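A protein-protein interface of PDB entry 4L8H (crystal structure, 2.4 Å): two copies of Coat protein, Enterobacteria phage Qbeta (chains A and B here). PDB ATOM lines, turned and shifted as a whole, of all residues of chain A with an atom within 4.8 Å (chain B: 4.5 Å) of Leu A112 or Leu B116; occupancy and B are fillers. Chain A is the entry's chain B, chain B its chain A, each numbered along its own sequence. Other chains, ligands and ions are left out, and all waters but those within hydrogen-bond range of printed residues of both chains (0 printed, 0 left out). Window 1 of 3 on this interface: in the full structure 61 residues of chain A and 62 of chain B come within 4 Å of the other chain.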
ATOM      1  N   VAL A  92     -30.226  11.335  12.851  1.00  0.00           N
ATOM      2  CA  VAL A  92     -30.591  12.096  11.652  1.00  0.00           C
ATOM      3  C   VAL A  92     -31.909  11.591  11.017  1.00  0.00           C
ATOM      4  O   VAL A  92     -32.095  10.393  10.785  1.00  0.00           O
ATOM      5  CB  VAL A  92     -29.432  12.129  10.603  1.00  0.00           C
ATOM      6  CG1 VAL A  92     -29.699  13.184   9.525  1.00  0.00           C
ATOM      7  CG2 VAL A  92     -28.111  12.499  11.282  1.00  0.00           C
ATOM      8  N   PHE A  94     -34.221  12.478   7.577  1.00  0.00           N
ATOM      9  CA  PHE A  94     -34.369  13.211   6.327  1.00  0.00           C
ATOM     10  C   PHE A  94     -35.811  13.083   5.881  1.00  0.00           C
ATOM     11  O   PHE A  94     -36.450  12.057   6.129  1.00  0.00           O
ATOM     12  CB  PHE A  94     -33.452  12.644   5.244  1.00  0.00           C
ATOM     13  CG  PHE A  94     -31.973  12.769   5.542  1.00  0.00           C
ATOM     14  CD1 PHE A  94     -31.301  11.760   6.228  1.00  0.00           C
ATOM     15  CD2 PHE A  94     -31.246  13.876   5.085  1.00  0.00           C
ATOM     16  CE1 PHE A  94     -29.924  11.865   6.472  1.00  0.00           C
ATOM     17  CE2 PHE A  94     -29.885  13.979   5.293  1.00  0.00           C
ATOM     18  CZ  PHE A  94     -29.210  12.977   5.988  1.00  0.00           C
ATOM     19  N   VAL A 108     -28.727  17.941   0.072  1.00  0.00           N
ATOM     20  CA  VAL A 108     -28.924  17.910   1.516  1.00  0.00           C
ATOM     21  C   VAL A 108     -27.880  17.020   2.211  1.00  0.00           C
ATOM     22  O   VAL A 108     -27.227  17.462   3.147  1.00  0.00           O
ATOM     23  CB  VAL A 108     -30.283  17.401   1.869  1.00  0.00           C
ATOM     24  CG1 VAL A 108     -30.375  17.245   3.380  1.00  0.00           C
ATOM     25  CG2 VAL A 108     -31.345  18.376   1.344  1.00  0.00           C
ATOM     26  N   ARG A 109     -27.677  15.808   1.697  1.00  0.00           N
ATOM     27  CA  ARG A 109     -26.677  14.907   2.241  1.00  0.00           C
ATOM     28  C   ARG A 109     -25.254  15.526   2.314  1.00  0.00           C
ATOM     29  O   ARG A 109     -24.566  15.431   3.350  1.00  0.00           O
ATOM     30  CB  ARG A 109     -26.668  13.569   1.456  1.00  0.00           C
ATOM     31  CG  ARG A 109     -25.448  12.719   1.733  1.00  0.00           C
ATOM     32  CD  ARG A 109     -25.419  11.399   0.977  1.00  0.00           C
ATOM     33  NE  ARG A 109     -25.161  11.616  -0.436  1.00  0.00           N
ATOM     34  CZ  ARG A 109     -23.959  11.875  -0.934  1.00  0.00           C
ATOM     35  NH1 ARG A 109     -22.911  11.932  -0.131  1.00  0.00           N
ATOM     36  NH2 ARG A 109     -23.806  12.030  -2.249  1.00  0.00           N
ATOM     37  N   THR A 110     -24.808  16.101   1.202  1.00  0.00           N
ATOM     38  CA  THR A 110     -23.466  16.670   1.095  1.00  0.00           C
ATOM     39  C   THR A 110     -23.378  18.038   1.771  1.00  0.00           C
ATOM     40  O   THR A 110     -22.319  18.408   2.229  1.00  0.00           O
ATOM     41  CB  THR A 110     -22.997  16.829  -0.357  1.00  0.00           C
ATOM     42  OG1 THR A 110     -23.963  17.599  -1.087  1.00  0.00           O
ATOM     43  CG2 THR A 110     -22.780  15.427  -1.003  1.00  0.00           C
ATOM     44  N   GLU A 111     -24.501  18.758   1.834  1.00  0.00           N
ATOM     45  CA  GLU A 111     -24.609  19.994   2.613  1.00  0.00           C
ATOM     46  C   GLU A 111     -24.322  19.734   4.112  1.00  0.00           C
ATOM     47  O   GLU A 111     -23.471  20.404   4.687  1.00  0.00           O
ATOM     48  CB  GLU A 111     -26.014  20.632   2.465  1.00  0.00           C
ATOM     49  CG  GLU A 111     -26.066  22.032   3.016  1.00  0.00           C
ATOM     50  CD  GLU A 111     -27.457  22.603   3.177  1.00  0.00           C
ATOM     51  OE1 GLU A 111     -28.377  22.281   2.397  1.00  0.00           O
ATOM     52  OE2 GLU A 111     -27.638  23.437   4.092  1.00  0.00           O
ATOM     53  N   LEU A 112     -25.054  18.778   4.703  1.00  0.00           N
ATOM     54  CA  LEU A 112     -24.907  18.356   6.077  1.00  0.00           C
ATOM     55  C   LEU A 112     -23.479  17.871   6.396  1.00  0.00           C
ATOM     56  O   LEU A 112     -22.908  18.282   7.405  1.00  0.00           O
ATOM     57  CB  LEU A 112     -25.920  17.265   6.414  1.00  0.00           C
ATOM     58  CG  LEU A 112     -25.888  16.764   7.882  1.00  0.00           C
ATOM     59  CD1 LEU A 112     -26.116  17.923   8.931  1.00  0.00           C
ATOM     60  CD2 LEU A 112     -26.971  15.694   8.090  1.00  0.00           C
ATOM     61  N   ALA A 113     -22.896  17.046   5.518  1.00  0.00           N
ATOM     62  CA  ALA A 113     -21.537  16.601   5.712  1.00  0.00           C
ATOM     63  C   ALA A 113     -20.641  17.807   5.825  1.00  0.00           C
ATOM     64  O   ALA A 113     -19.773  17.820   6.693  1.00  0.00           O
ATOM     65  CB  ALA A 113     -21.056  15.730   4.567  1.00  0.00           C
ATOM     66  N   ALA A 114     -20.818  18.792   4.934  1.00  0.00           N
ATOM     67  CA  ALA A 114     -19.938  19.986   4.921  1.00  0.00           C
ATOM     68  C   ALA A 114     -20.218  20.872   6.147  1.00  0.00           C
ATOM     69  O   ALA A 114     -19.306  21.312   6.815  1.00  0.00           O
ATOM     70  CB  ALA A 114     -20.084  20.781   3.639  1.00  0.00           C
ATOM     71  N   LEU A 115     -21.479  21.094   6.437  1.00  0.00           N
ATOM     72  CA  LEU A 115     -21.848  21.813   7.615  1.00  0.00           C
ATOM     73  C   LEU A 115     -21.141  21.262   8.895  1.00  0.00           C
ATOM     74  O   LEU A 115     -20.619  22.028   9.734  1.00  0.00           O
ATOM     75  CB  LEU A 115     -23.356  21.784   7.717  1.00  0.00           C
ATOM     76  CG  LEU A 115     -23.973  22.715   8.757  1.00  0.00           C
ATOM     77  CD1 LEU A 115     -23.606  24.226   8.533  1.00  0.00           C
ATOM     78  CD2 LEU A 115     -25.488  22.475   8.876  1.00  0.00           C
ATOM     79  N   LEU A 116     -21.057  19.934   8.990  1.00  0.00           N
ATOM     80  CA  LEU A 116     -20.512  19.278  10.158  1.00  0.00           C
ATOM     81  C   LEU A 116     -19.001  19.563  10.276  1.00  0.00           C
ATOM     82  O   LEU A 116     -18.383  19.300  11.328  1.00  0.00           O
ATOM     83  CB  LEU A 116     -20.802  17.764  10.116  1.00  0.00           C
ATOM     84  CG  LEU A 116     -22.223  17.291  10.413  1.00  0.00           C
ATOM     85  CD1 LEU A 116     -22.390  15.790  10.103  1.00  0.00           C
ATOM     86  CD2 LEU A 116     -22.627  17.586  11.855  1.00  0.00           C
ATOM     87  N   ILE B  68     -31.996  21.599   8.522  1.00  0.00           N
ATOM     88  CA  ILE B  68     -31.813  22.073   7.169  1.00  0.00           C
ATOM     89  C   ILE B  68     -33.201  22.127   6.516  1.00  0.00           C
ATOM     90  O   ILE B  68     -34.035  21.218   6.693  1.00  0.00           O
ATOM     91  CB  ILE B  68     -30.832  21.185   6.380  1.00  0.00           C
ATOM     92  CG1 ILE B  68     -29.416  21.330   6.966  1.00  0.00           C
ATOM     93  CG2 ILE B  68     -30.858  21.490   4.814  1.00  0.00           C
ATOM     94  CD1 ILE B  68     -28.317  20.489   6.261  1.00  0.00           C
ATOM     95  N   VAL B  92     -31.164  16.927  12.702  1.00  0.00           N
ATOM     96  CA  VAL B  92     -30.045  16.314  13.407  1.00  0.00           C
ATOM     97  C   VAL B  92     -30.057  16.665  14.906  1.00  0.00           C
ATOM     98  O   VAL B  92     -30.001  17.844  15.274  1.00  0.00           O
ATOM     99  CB  VAL B  92     -28.671  16.801  12.845  1.00  0.00           C
ATOM    100  CG1 VAL B  92     -27.589  15.819  13.176  1.00  0.00           C
ATOM    101  CG2 VAL B  92     -28.720  17.000  11.367  1.00  0.00           C
ATOM    102  N   LEU B 112     -20.266  11.040  11.777  1.00  0.00           N
ATOM    103  CA  LEU B 112     -21.405  11.349  10.952  1.00  0.00           C
ATOM    104  C   LEU B 112     -20.992  11.938   9.584  1.00  0.00           C
ATOM    105  O   LEU B 112     -21.455  11.459   8.551  1.00  0.00           O
ATOM    106  CB  LEU B 112     -22.405  12.233  11.645  1.00  0.00           C
ATOM    107  CG  LEU B 112     -23.684  12.498  10.838  1.00  0.00           C
ATOM    108  CD1 LEU B 112     -24.429  11.231  10.350  1.00  0.00           C
ATOM    109  CD2 LEU B 112     -24.651  13.382  11.660  1.00  0.00           C
ATOM    110  N   ALA B 113     -20.118  12.942   9.549  1.00  0.00           N
ATOM    111  CA  ALA B 113     -19.813  13.552   8.223  1.00  0.00           C
ATOM    112  C   ALA B 113     -19.277  12.475   7.256  1.00  0.00           C
ATOM    113  O   ALA B 113     -19.606  12.490   6.098  1.00  0.00           O
ATOM    114  CB  ALA B 113     -18.842  14.708   8.323  1.00  0.00           C
ATOM    115  N   ALA B 114     -18.413  11.594   7.738  1.00  0.00           N
ATOM    116  CA  ALA B 114     -17.845  10.557   6.904  1.00  0.00           C
ATOM    117  C   ALA B 114     -18.947   9.536   6.462  1.00  0.00           C
ATOM    118  O   ALA B 114     -19.041   9.135   5.298  1.00  0.00           O
ATOM    119  CB  ALA B 114     -16.750   9.865   7.644  1.00  0.00           C
ATOM    120  N   LEU B 115     -19.816   9.187   7.396  1.00  0.00           N
ATOM    121  CA  LEU B 115     -20.900   8.259   7.135  1.00  0.00           C
ATOM    122  C   LEU B 115     -21.682   8.750   5.928  1.00  0.00           C
ATOM    123  O   LEU B 115     -22.077   7.947   5.065  1.00  0.00           O
ATOM    124  CB  LEU B 115     -21.777   8.139   8.380  1.00  0.00           C
ATOM    125  CG  LEU B 115     -22.634   6.851   8.548  1.00  0.00           C
ATOM    126  CD1 LEU B 115     -21.890   5.508   8.302  1.00  0.00           C
ATOM    127  CD2 LEU B 115     -23.363   6.827   9.904  1.00  0.00           C
ATOM    128  N   LEU B 116     -21.839  10.067   5.826  1.00  0.00           N
ATOM    129  CA  LEU B 116     -22.715  10.644   4.824  1.00  0.00           C
ATOM    130  C   LEU B 116     -22.069  10.628   3.417  1.00  0.00           C
ATOM    131  O   LEU B 116     -22.742  10.835   2.423  1.00  0.00           O
ATOM    132  CB  LEU B 116     -23.129  12.062   5.217  1.00  0.00           C
ATOM    133  CG  LEU B 116     -24.065  12.261   6.409  1.00  0.00           C
ATOM    134  CD1 LEU B 116     -24.163  13.757   6.739  1.00  0.00           C
ATOM    135  CD2 LEU B 116     -25.451  11.685   6.155  1.00  0.00           C
ATOM    136  N   ALA B 117     -20.780  10.345   3.364  1.00  0.00           N
ATOM    137  CA  ALA B 117     -20.078  10.081   2.126  1.00  0.00           C
ATOM    138  C   ALA B 117     -19.943   8.570   1.767  1.00  0.00           C
ATOM    139  O   ALA B 117     -19.324   8.236   0.746  1.00  0.00           O
ATOM    140  CB  ALA B 117     -18.692  10.766   2.148  1.00  0.00           C
ATOM    141  N   SER B 118     -20.527   7.654   2.553  1.00  0.00           N
ATOM    142  CA  SER B 118     -20.279   6.192   2.297  1.00  0.00           C
ATOM    143  C   SER B 118     -21.247   5.647   1.249  1.00  0.00           C
ATOM    144  O   SER B 118     -22.338   6.167   1.140  1.00  0.00           O
ATOM    145  CB  SER B 118     -20.444   5.378   3.595  1.00  0.00           C
ATOM    146  OG  SER B 118     -21.811   5.392   4.023  1.00  0.00           O
ATOM    147  N   LEU B 121     -24.926   5.324   2.613  1.00  0.00           N
ATOM    148  CA  LEU B 121     -25.768   6.483   2.796  1.00  0.00           C
ATOM    149  C   LEU B 121     -26.086   7.161   1.448  1.00  0.00           C
ATOM    150  O   LEU B 121     -27.178   7.723   1.277  1.00  0.00           O
ATOM    151  CB  LEU B 121     -25.202   7.449   3.863  1.00  0.00           C
ATOM    152  CG  LEU B 121     -25.577   7.150   5.339  1.00  0.00           C
ATOM    153  CD1 LEU B 121     -27.072   6.977   5.470  1.00  0.00           C
ATOM    154  CD2 LEU B 121     -24.963   5.858   5.831  1.00  0.00           C
ATOM    155  N   ILE B 122     -25.169   7.082   0.489  1.00  0.00           N
ATOM    156  CA  ILE B 122     -25.452   7.528  -0.867  1.00  0.00           C
ATOM    157  C   ILE B 122     -26.671   6.752  -1.433  1.00  0.00           C
ATOM    158  O   ILE B 122     -27.647   7.350  -1.939  1.00  0.00           O
ATOM    159  CB  ILE B 122     -24.162   7.371  -1.762  1.00  0.00           C
ATOM    160  CG1 ILE B 122     -23.071   8.381  -1.292  1.00  0.00           C
ATOM    161  CG2 ILE B 122     -24.518   7.495  -3.282  1.00  0.00           C
ATOM    162  CD1 ILE B 122     -21.706   8.268  -2.013  1.00  0.00           C
ATOM    163  N   ILE B 125     -29.925   7.707   0.728  1.00  0.00           N
ATOM    164  CA  ILE B 125     -30.418   9.058   0.622  1.00  0.00           C
ATOM    165  C   ILE B 125     -30.602   9.446  -0.855  1.00  0.00           C
ATOM    166  O   ILE B 125     -31.696   9.828  -1.242  1.00  0.00           O
ATOM    167  CB  ILE B 125     -29.510  10.044   1.345  1.00  0.00           C
ATOM    168  CG1 ILE B 125     -29.570   9.850   2.872  1.00  0.00           C
ATOM    169  CG2 ILE B 125     -29.860  11.496   0.971  1.00  0.00           C
ATOM    170  CD1 ILE B 125     -28.270  10.353   3.576  1.00  0.00           C
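The backbone carbonyl oxygen of Leu B116 sits at hydrogen-bond distance from the guanidinium group of Arg A109, at 2.8 Å.
Leu B112 touches Val A92 (CD2 to CG2, 3.6 Å).
Phe A94 touches Leu B116.
CD1 of Ile B125 touches CE1 of Phe A94, 3.7 Å away.
Arg A109 touches Ile B125.
CG2 of Ile B68 touches OE1 of Glu A111 (3.6 Å).
CG2 of Val B92 touches CD1 of Leu A112, at 3.7 Å.
Leu B116 touches Leu A112 (CD1 to CG, 3.7 Å).
Ala B113 touches Ala A113 (CB to O, 3.6 Å).
N of Ala A113 touches CD1 of Leu B116 (3.7 Å).
Leu B112 touches Leu A116 (CG to CD1, 3.6 Å).
Of the printed residues of chain B, Arg A109 touches Leu B116 (2.8 Å), Ile B122 (3.6 Å) and Ile B125 (3.8 Å).
Of the printed residues of chain B, Leu A112 touches Val B92 (3.7 Å) and Leu B116 (3.7 Å).
Printed residues of chain B within 4 Å of Leu A116: Leu B112 and Ala B113.
Printed residues of chain A within 4 Å of Val B92: Val A92 and Leu A112.
Printed residues of chain A within 4 Å of Leu B112: Val A92 and Leu A116.
Of chain A, only Phe A94 (3.98 Å), Arg A109 (2.8 Å), Leu A112 (3.7 Å) and Ala A113 (3.7 Å) come within 4 Å of Leu B116.
Leu B121 touches none of the printed residues of chain A.
The nearest residue of chain A that does not touch Leu B116 is Leu A116 (4.3 Å).
Printed residues of chain A that touch a printed residue of chain B: Val A92, Phe A94, Arg A109, Glu A111, Leu A112, Ala A113 and Leu A116.
Among the printed residues, 14 pairs touch across the chains.
Among the printed residues, no Asp or Glu carboxylate lies within 4 Å of a Lys or Arg side-chain nitrogen of the other chain.
Val A92 touches Leu B112, and with the chains exchanged Leu A112 touches Val B92.
Leu A112 touches Leu B116, and with the chains exchanged Leu A116 touches Leu B112.
Ala A113 touches its own counterpart, Ala B113.
Ala A113 touches Leu B116, and with the chains exchanged Leu A116 touches Ala B113.
Positions printed for both chains: 92, 112, 113, 114, 115 and 116.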
